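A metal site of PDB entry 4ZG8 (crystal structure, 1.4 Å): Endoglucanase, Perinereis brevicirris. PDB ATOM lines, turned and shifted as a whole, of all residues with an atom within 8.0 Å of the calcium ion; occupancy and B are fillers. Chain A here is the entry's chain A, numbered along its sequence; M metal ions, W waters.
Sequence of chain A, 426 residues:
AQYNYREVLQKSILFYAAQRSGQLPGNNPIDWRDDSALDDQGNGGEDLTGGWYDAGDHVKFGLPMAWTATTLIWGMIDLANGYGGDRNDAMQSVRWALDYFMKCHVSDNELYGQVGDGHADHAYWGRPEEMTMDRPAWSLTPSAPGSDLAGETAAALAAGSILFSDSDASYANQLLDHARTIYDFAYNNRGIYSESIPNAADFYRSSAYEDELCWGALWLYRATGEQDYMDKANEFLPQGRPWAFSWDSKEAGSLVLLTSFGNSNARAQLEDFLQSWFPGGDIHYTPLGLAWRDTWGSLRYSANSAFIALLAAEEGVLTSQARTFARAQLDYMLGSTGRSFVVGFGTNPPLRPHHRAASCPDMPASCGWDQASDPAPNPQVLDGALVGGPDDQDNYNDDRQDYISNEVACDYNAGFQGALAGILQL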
ATOM      1  N   LEU A  63      23.325  31.527 -21.668  1.00  0.00           N
ATOM      2  CA  LEU A  63      23.691  30.126 -21.999  1.00  0.00           C
ATOM      3  C   LEU A  63      23.682  29.855 -23.519  1.00  0.00           C
ATOM      4  O   LEU A  63      24.739  29.474 -24.031  1.00  0.00           O
ATOM      5  CB  LEU A  63      22.912  29.093 -21.199  1.00  0.00           C
ATOM      6  CG  LEU A  63      23.215  27.630 -21.511  1.00  0.00           C
ATOM      7  CD1 LEU A  63      24.692  27.274 -21.329  1.00  0.00           C
ATOM      8  CD2 LEU A  63      22.330  26.731 -20.690  1.00  0.00           C
ATOM      9  N   SER A 147      26.890  26.588 -12.947  1.00  0.00           N
ATOM     10  CA  SER A 147      28.033  25.923 -13.564  1.00  0.00           C
ATOM     11  C   SER A 147      27.912  25.715 -15.058  1.00  0.00           C
ATOM     12  O   SER A 147      28.915  25.608 -15.749  1.00  0.00           O
ATOM     13  CB  SER A 147      28.285  24.600 -12.859  1.00  0.00           C
ATOM     14  OG  SER A 147      28.423  24.764 -11.453  1.00  0.00           O
ATOM     15  N   ASP A 148      26.664  25.566 -15.485  1.00  0.00           N
ATOM     16  CA  ASP A 148      26.315  25.390 -16.883  1.00  0.00           C
ATOM     17  C   ASP A 148      26.617  26.694 -17.683  1.00  0.00           C
ATOM     18  O   ASP A 148      27.422  26.714 -18.590  1.00  0.00           O
ATOM     19  CB  ASP A 148      24.852  24.895 -17.045  1.00  0.00           C
ATOM     20  CG  ASP A 148      23.892  25.462 -16.017  1.00  0.00           C
ATOM     21  OD1 ASP A 148      24.173  26.541 -15.440  1.00  0.00           O
ATOM     22  OD2 ASP A 148      22.858  24.808 -15.793  1.00  0.00           O
ATOM     23  N   LEU A 149      25.977  27.782 -17.316  1.00  0.00           N
ATOM     24  CA  LEU A 149      26.183  29.035 -17.992  1.00  0.00           C
ATOM     25  C   LEU A 149      27.637  29.488 -17.856  1.00  0.00           C
ATOM     26  O   LEU A 149      28.275  29.917 -18.828  1.00  0.00           O
ATOM     27  CB  LEU A 149      25.203  30.075 -17.491  1.00  0.00           C
ATOM     28  CG  LEU A 149      25.136  31.391 -18.283  1.00  0.00           C
ATOM     29  CD1 LEU A 149      23.748  32.025 -18.161  1.00  0.00           C
ATOM     30  CD2 LEU A 149      26.205  32.379 -17.797  1.00  0.00           C
ATOM     31  N   GLU A 152      30.046  27.206 -19.891  1.00  0.00           N
ATOM     32  CA  GLU A 152      29.924  27.480 -21.313  1.00  0.00           C
ATOM     33  C   GLU A 152      30.607  28.795 -21.661  1.00  0.00           C
ATOM     34  O   GLU A 152      31.258  28.946 -22.703  1.00  0.00           O
ATOM     35  CB  GLU A 152      28.469  27.522 -21.757  1.00  0.00           C
ATOM     36  CG  GLU A 152      28.322  27.639 -23.261  1.00  0.00           C
ATOM     37  CD  GLU A 152      28.835  26.410 -23.975  1.00  0.00           C
ATOM     38  OE1 GLU A 152      28.348  25.317 -23.643  1.00  0.00           O
ATOM     39  OE2 GLU A 152      29.716  26.524 -24.893  1.00  0.00           O
ATOM     40  N   ILE A 192      22.647  24.792 -11.130  1.00  0.00           N
ATOM     41  CA  ILE A 192      21.971  24.973 -12.392  1.00  0.00           C
ATOM     42  C   ILE A 192      21.609  26.421 -12.520  1.00  0.00           C
ATOM     43  O   ILE A 192      20.893  26.980 -11.632  1.00  0.00           O
ATOM     44  CB  ILE A 192      20.660  24.102 -12.394  1.00  0.00           C
ATOM     45  CG1 ILE A 192      21.042  22.641 -12.372  1.00  0.00           C
ATOM     46  CG2 ILE A 192      19.796  24.473 -13.560  1.00  0.00           C
ATOM     47  CD1 ILE A 192      21.513  22.142 -13.690  1.00  0.00           C
ATOM     48  N   ARG A 205      15.707  26.500 -19.844  1.00  0.00           N
ATOM     49  CA  ARG A 205      15.885  25.647 -18.673  1.00  0.00           C
ATOM     50  C   ARG A 205      17.008  24.705 -18.914  1.00  0.00           C
ATOM     51  O   ARG A 205      16.975  23.903 -19.873  1.00  0.00           O
ATOM     52  CB  ARG A 205      14.605  24.876 -18.401  1.00  0.00           C
ATOM     53  CG  ARG A 205      14.632  23.935 -17.220  1.00  0.00           C
ATOM     54  CD  ARG A 205      13.412  23.060 -17.325  1.00  0.00           C
ATOM     55  NE  ARG A 205      13.403  22.115 -16.237  1.00  0.00           N
ATOM     56  CZ  ARG A 205      12.626  21.052 -16.150  1.00  0.00           C
ATOM     57  NH1 ARG A 205      11.810  20.715 -17.156  1.00  0.00           N
ATOM     58  NH2 ARG A 205      12.703  20.317 -15.066  1.00  0.00           N
ATOM     59  N   SER A 206      17.993  24.701 -18.053  1.00  0.00           N
ATOM     60  CA  SER A 206      19.148  23.808 -18.195  1.00  0.00           C
ATOM     61  C   SER A 206      18.826  22.467 -17.584  1.00  0.00           C
ATOM     62  O   SER A 206      18.355  22.380 -16.433  1.00  0.00           O
ATOM     63  CB  SER A 206      20.391  24.393 -17.503  1.00  0.00           C
ATOM     64  OG  SER A 206      21.376  23.387 -17.339  1.00  0.00           O
ATOM     65  N   SER A 207      19.117  21.389 -18.309  1.00  0.00           N
ATOM     66  CA  SER A 207      18.884  20.014 -17.807  1.00  0.00           C
ATOM     67  C   SER A 207      19.977  19.475 -16.883  1.00  0.00           C
ATOM     68  O   SER A 207      19.717  18.559 -16.101  1.00  0.00           O
ATOM     69  CB  SER A 207      18.653  19.041 -18.985  1.00  0.00           C
ATOM     70  OG  SER A 207      19.736  18.975 -19.869  1.00  0.00           O
ATOM     71  N   ALA A 208      21.180  20.007 -16.986  1.00  0.00           N
ATOM     72  CA  ALA A 208      22.336  19.503 -16.233  1.00  0.00           C
ATOM     73  C   ALA A 208      23.517  20.416 -16.486  1.00  0.00           C
ATOM     74  O   ALA A 208      23.560  21.047 -17.545  1.00  0.00           O
ATOM     75  CB  ALA A 208      22.726  18.082 -16.641  1.00  0.00           C
ATOM     76  N   TYR A 209      24.467  20.436 -15.528  1.00  0.00           N
ATOM     77  CA  TYR A 209      25.669  21.226 -15.702  1.00  0.00           C
ATOM     78  C   TYR A 209      26.935  20.430 -15.845  1.00  0.00           C
ATOM     79  O   TYR A 209      27.947  21.004 -16.232  1.00  0.00           O
ATOM     80  CB  TYR A 209      25.802  22.250 -14.571  1.00  0.00           C
ATOM     81  CG  TYR A 209      26.000  21.628 -13.195  1.00  0.00           C
ATOM     82  CD1 TYR A 209      27.184  21.031 -12.822  1.00  0.00           C
ATOM     83  CD2 TYR A 209      24.973  21.625 -12.301  1.00  0.00           C
ATOM     84  CE1 TYR A 209      27.335  20.423 -11.588  1.00  0.00           C
ATOM     85  CE2 TYR A 209      25.108  21.019 -11.062  1.00  0.00           C
ATOM     86  CZ  TYR A 209      26.287  20.433 -10.709  1.00  0.00           C
ATOM     87  OH  TYR A 209      26.375  19.847  -9.482  1.00  0.00           O
ATOM     88  N   GLU A 210      26.938  19.136 -15.553  1.00  0.00           N
ATOM     89  CA  GLU A 210      28.227  18.415 -15.580  1.00  0.00           C
ATOM     90  C   GLU A 210      28.812  18.375 -17.006  1.00  0.00           C
ATOM     91  O   GLU A 210      30.020  18.360 -17.165  1.00  0.00           O
ATOM     92  CB  GLU A 210      28.079  17.028 -15.034  1.00  0.00           C
ATOM     93  CG  GLU A 210      27.799  16.933 -13.547  1.00  0.00           C
ATOM     94  CD  GLU A 210      26.301  17.089 -13.136  1.00  0.00           C
ATOM     95  OE1 GLU A 210      25.311  17.490 -13.912  1.00  0.00           O
ATOM     96  OE2 GLU A 210      26.103  16.847 -11.910  1.00  0.00           O
ATOM     97  N   ASP A 211      27.935  18.386 -18.009  1.00  0.00           N
ATOM     98  CA  ASP A 211      28.433  18.341 -19.386  1.00  0.00           C
ATOM     99  C   ASP A 211      29.168  19.634 -19.754  1.00  0.00           C
ATOM    100  O   ASP A 211      30.143  19.618 -20.483  1.00  0.00           O
ATOM    101  CB  ASP A 211      27.331  18.022 -20.364  1.00  0.00           C
ATOM    102  CG  ASP A 211      26.133  18.966 -20.253  1.00  0.00           C
ATOM    103  OD1 ASP A 211      25.510  19.014 -19.153  1.00  0.00           O
ATOM    104  OD2 ASP A 211      25.754  19.653 -21.263  1.00  0.00           O
ATOM    105  N   GLU A 212      28.754  20.774 -19.174  1.00  0.00           N
ATOM    106  CA  GLU A 212      29.470  22.043 -19.388  1.00  0.00           C
ATOM    107  C   GLU A 212      30.765  22.032 -18.625  1.00  0.00           C
ATOM    108  O   GLU A 212      31.725  22.663 -19.085  1.00  0.00           O
ATOM    109  CB  GLU A 212      28.667  23.288 -18.995  1.00  0.00           C
ATOM    110  CG  GLU A 212      27.581  23.626 -20.012  1.00  0.00           C
ATOM    111  CD  GLU A 212      26.338  22.776 -19.912  1.00  0.00           C
ATOM    112  OE1 GLU A 212      26.125  22.050 -18.904  1.00  0.00           O
ATOM    113  OE2 GLU A 212      25.532  22.778 -20.889  1.00  0.00           O
ATOM    114  N   LEU A 213      30.794  21.405 -17.427  1.00  0.00           N
ATOM    115  CA  LEU A 213      32.066  21.272 -16.718  1.00  0.00           C
ATOM    116  C   LEU A 213      33.118  20.447 -17.506  1.00  0.00           C
ATOM    117  O   LEU A 213      34.304  20.802 -17.580  1.00  0.00           O
ATOM    118  CB  LEU A 213      31.887  20.801 -15.301  1.00  0.00           C
ATOM    119  CG  LEU A 213      31.156  21.756 -14.354  1.00  0.00           C
ATOM    120  CD1 LEU A 213      31.020  21.124 -12.985  1.00  0.00           C
ATOM    121  CD2 LEU A 213      31.857  23.088 -14.239  1.00  0.00           C
ATOM    122  N   SER A 246      23.452  20.592 -28.544  1.00  0.00           N
ATOM    123  CA  SER A 246      22.672  21.831 -28.524  1.00  0.00           C
ATOM    124  C   SER A 246      23.230  22.764 -27.456  1.00  0.00           C
ATOM    125  O   SER A 246      24.159  22.401 -26.756  1.00  0.00           O
ATOM    126  CB  SER A 246      21.201  21.501 -28.210  1.00  0.00           C
ATOM    127  OG  SER A 246      21.072  21.202 -26.834  1.00  0.00           O
ATOM    128  N   TRP A 247      22.553  23.920 -27.321  1.00  0.00           N
ATOM    129  CA  TRP A 247      22.855  24.842 -26.236  1.00  0.00           C
ATOM    130  C   TRP A 247      22.741  24.226 -24.846  1.00  0.00           C
ATOM    131  O   TRP A 247      23.346  24.738 -23.910  1.00  0.00           O
ATOM    132  CB  TRP A 247      21.968  26.086 -26.334  1.00  0.00           C
ATOM    133  CG  TRP A 247      20.519  25.766 -26.129  1.00  0.00           C
ATOM    134  CD1 TRP A 247      19.596  25.521 -27.088  1.00  0.00           C
ATOM    135  CD2 TRP A 247      19.807  25.578 -24.879  1.00  0.00           C
ATOM    136  NE1 TRP A 247      18.398  25.201 -26.570  1.00  0.00           N
ATOM    137  CE2 TRP A 247      18.492  25.226 -25.203  1.00  0.00           C
ATOM    138  CE3 TRP A 247      20.146  25.695 -23.519  1.00  0.00           C
ATOM    139  CZ2 TRP A 247      17.535  24.943 -24.218  1.00  0.00           C
ATOM    140  CZ3 TRP A 247      19.213  25.431 -22.575  1.00  0.00           C
ATOM    141  CH2 TRP A 247      17.932  25.063 -22.904  1.00  0.00           C
ATOM    142  N   ASP A 248      21.975  23.145 -24.710  1.00  0.00           N
ATOM    143  CA  ASP A 248      21.710  22.494 -23.427  1.00  0.00           C
ATOM    144  C   ASP A 248      22.692  21.364 -23.166  1.00  0.00           C
ATOM    145  O   ASP A 248      23.089  21.146 -22.082  1.00  0.00           O
ATOM    146  CB  ASP A 248      20.290  21.987 -23.377  1.00  0.00           C
ATOM    147  CG  ASP A 248      19.881  21.420 -22.041  1.00  0.00           C
ATOM    148  OD1 ASP A 248      20.168  22.002 -20.999  1.00  0.00           O
ATOM    149  OD2 ASP A 248      19.191  20.340 -22.064  1.00  0.00           O
ATOM    150  N   SER A 249      22.998  20.578 -24.204  1.00  0.00           N
ATOM    151  CA  SER A 249      23.781  19.331 -24.051  1.00  0.00           C
ATOM    152  C   SER A 249      25.085  19.409 -24.813  1.00  0.00           C
ATOM    153  O   SER A 249      25.093  19.466 -26.056  1.00  0.00           O
ATOM    154  CB  SER A 249      23.005  18.128 -24.612  1.00  0.00           C
ATOM    155  OG  SER A 249      21.771  17.864 -23.946  1.00  0.00           O
ATOM    156  N   LYS A 250      26.183  19.309 -24.114  1.00  0.00           N
ATOM    157  CA  LYS A 250      27.518  19.415 -24.692  1.00  0.00           C
ATOM    158  C   LYS A 250      28.204  18.101 -24.946  1.00  0.00           C
ATOM    159  O   LYS A 250      29.263  18.083 -25.602  1.00  0.00           O
ATOM    160  CB  LYS A 250      28.446  20.269 -23.819  1.00  0.00           C
ATOM    161  CG  LYS A 250      27.819  21.579 -23.329  1.00  0.00           C
ATOM    162  CD  LYS A 250      27.356  22.426 -24.496  1.00  0.00           C
ATOM    163  CE  LYS A 250      25.992  23.046 -24.322  1.00  0.00           C
ATOM    164  NZ  LYS A 250      25.993  24.077 -23.246  1.00  0.00           N
ATOM    165  N   GLU A 251      27.617  17.003 -24.484  1.00  0.00           N
ATOM    166  CA  GLU A 251      28.328  15.709 -24.551  1.00  0.00           C
ATOM    167  C   GLU A 251      28.875  15.350 -25.943  1.00  0.00           C
ATOM    168  O   GLU A 251      29.997  14.868 -26.028  1.00  0.00           O
ATOM    169  CB  GLU A 251      27.423  14.574 -24.063  1.00  0.00           C
ATOM    170  CG  GLU A 251      27.102  14.616 -22.549  1.00  0.00           C
ATOM    171  CD  GLU A 251      25.880  15.344 -22.124  1.00  0.00           C
ATOM    172  OE1 GLU A 251      25.471  16.355 -22.748  1.00  0.00           O
ATOM    173  OE2 GLU A 251      25.307  14.879 -21.100  1.00  0.00           O
HETATM  174 CA    CA M   1      24.119  20.971 -19.917  1.00  0.00          CA
HETATM  175  O   HOH W   1      22.470  22.679 -19.720  1.00  0.00           O
HETATM  176  O   HOH W   2      22.536  19.175 -19.974  1.00  0.00           O
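The calcium ion is bound by water W1 (2.4 Å), water W2 (2.4 Å), the backbone carbonyl oxygen (O) of Asp 248 (2.4 Å), the backbone carbonyl oxygen (O) of Ala 208 (2.4 Å), the side-chain carboxylate (OE2) of Glu 212 (2.5 Å), the side-chain carboxylate (OE1) of Glu 212 (2.5 Å), the side-chain carboxylate (OD2) of Asp 211 (2.5 Å) and the side-chain carboxylate (OD1) of Asp 211 (2.5 Å).
The calcium ion has eight donor atoms within binding distance.
OG of Ser 207 sits at hydrogen-bond distance from OD2 of Asp 248, 2.6 Å away.
The backbone NH (N) of Asp 248 is in hydrogen-bond range of the side-chain hydroxyl (OG) of Ser 246, at 3.0 Å.
The backbone NH of Ala 208 is in hydrogen-bond range of the side-chain hydroxyl of Ser 206.
The side-chain carboxylate (OE2) of Glu 212 lies close to the side-chain amino group (NZ) of Lys 250 (2.7 Å).
The backbone NH of Lys 250 sits close to the side-chain carboxylate of Asp 211 (2.9 Å).
Water W2 bridges OG of Ser 207 (2.8 Å) and N of Ala 208 (3.4 Å).
Water W1 lies within hydrogen-bond range of the side-chain hydroxyl of Ser 206 (2.7 Å) and the side-chain carboxylate of Asp 248 (2.7 Å).
Within 4 Å of the calcium ion: Ala 208, Asp 211, Glu 212 and Asp 248.
The nearest printed residue that does not touch the calcium ion is Tyr 209 (4.4 Å).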
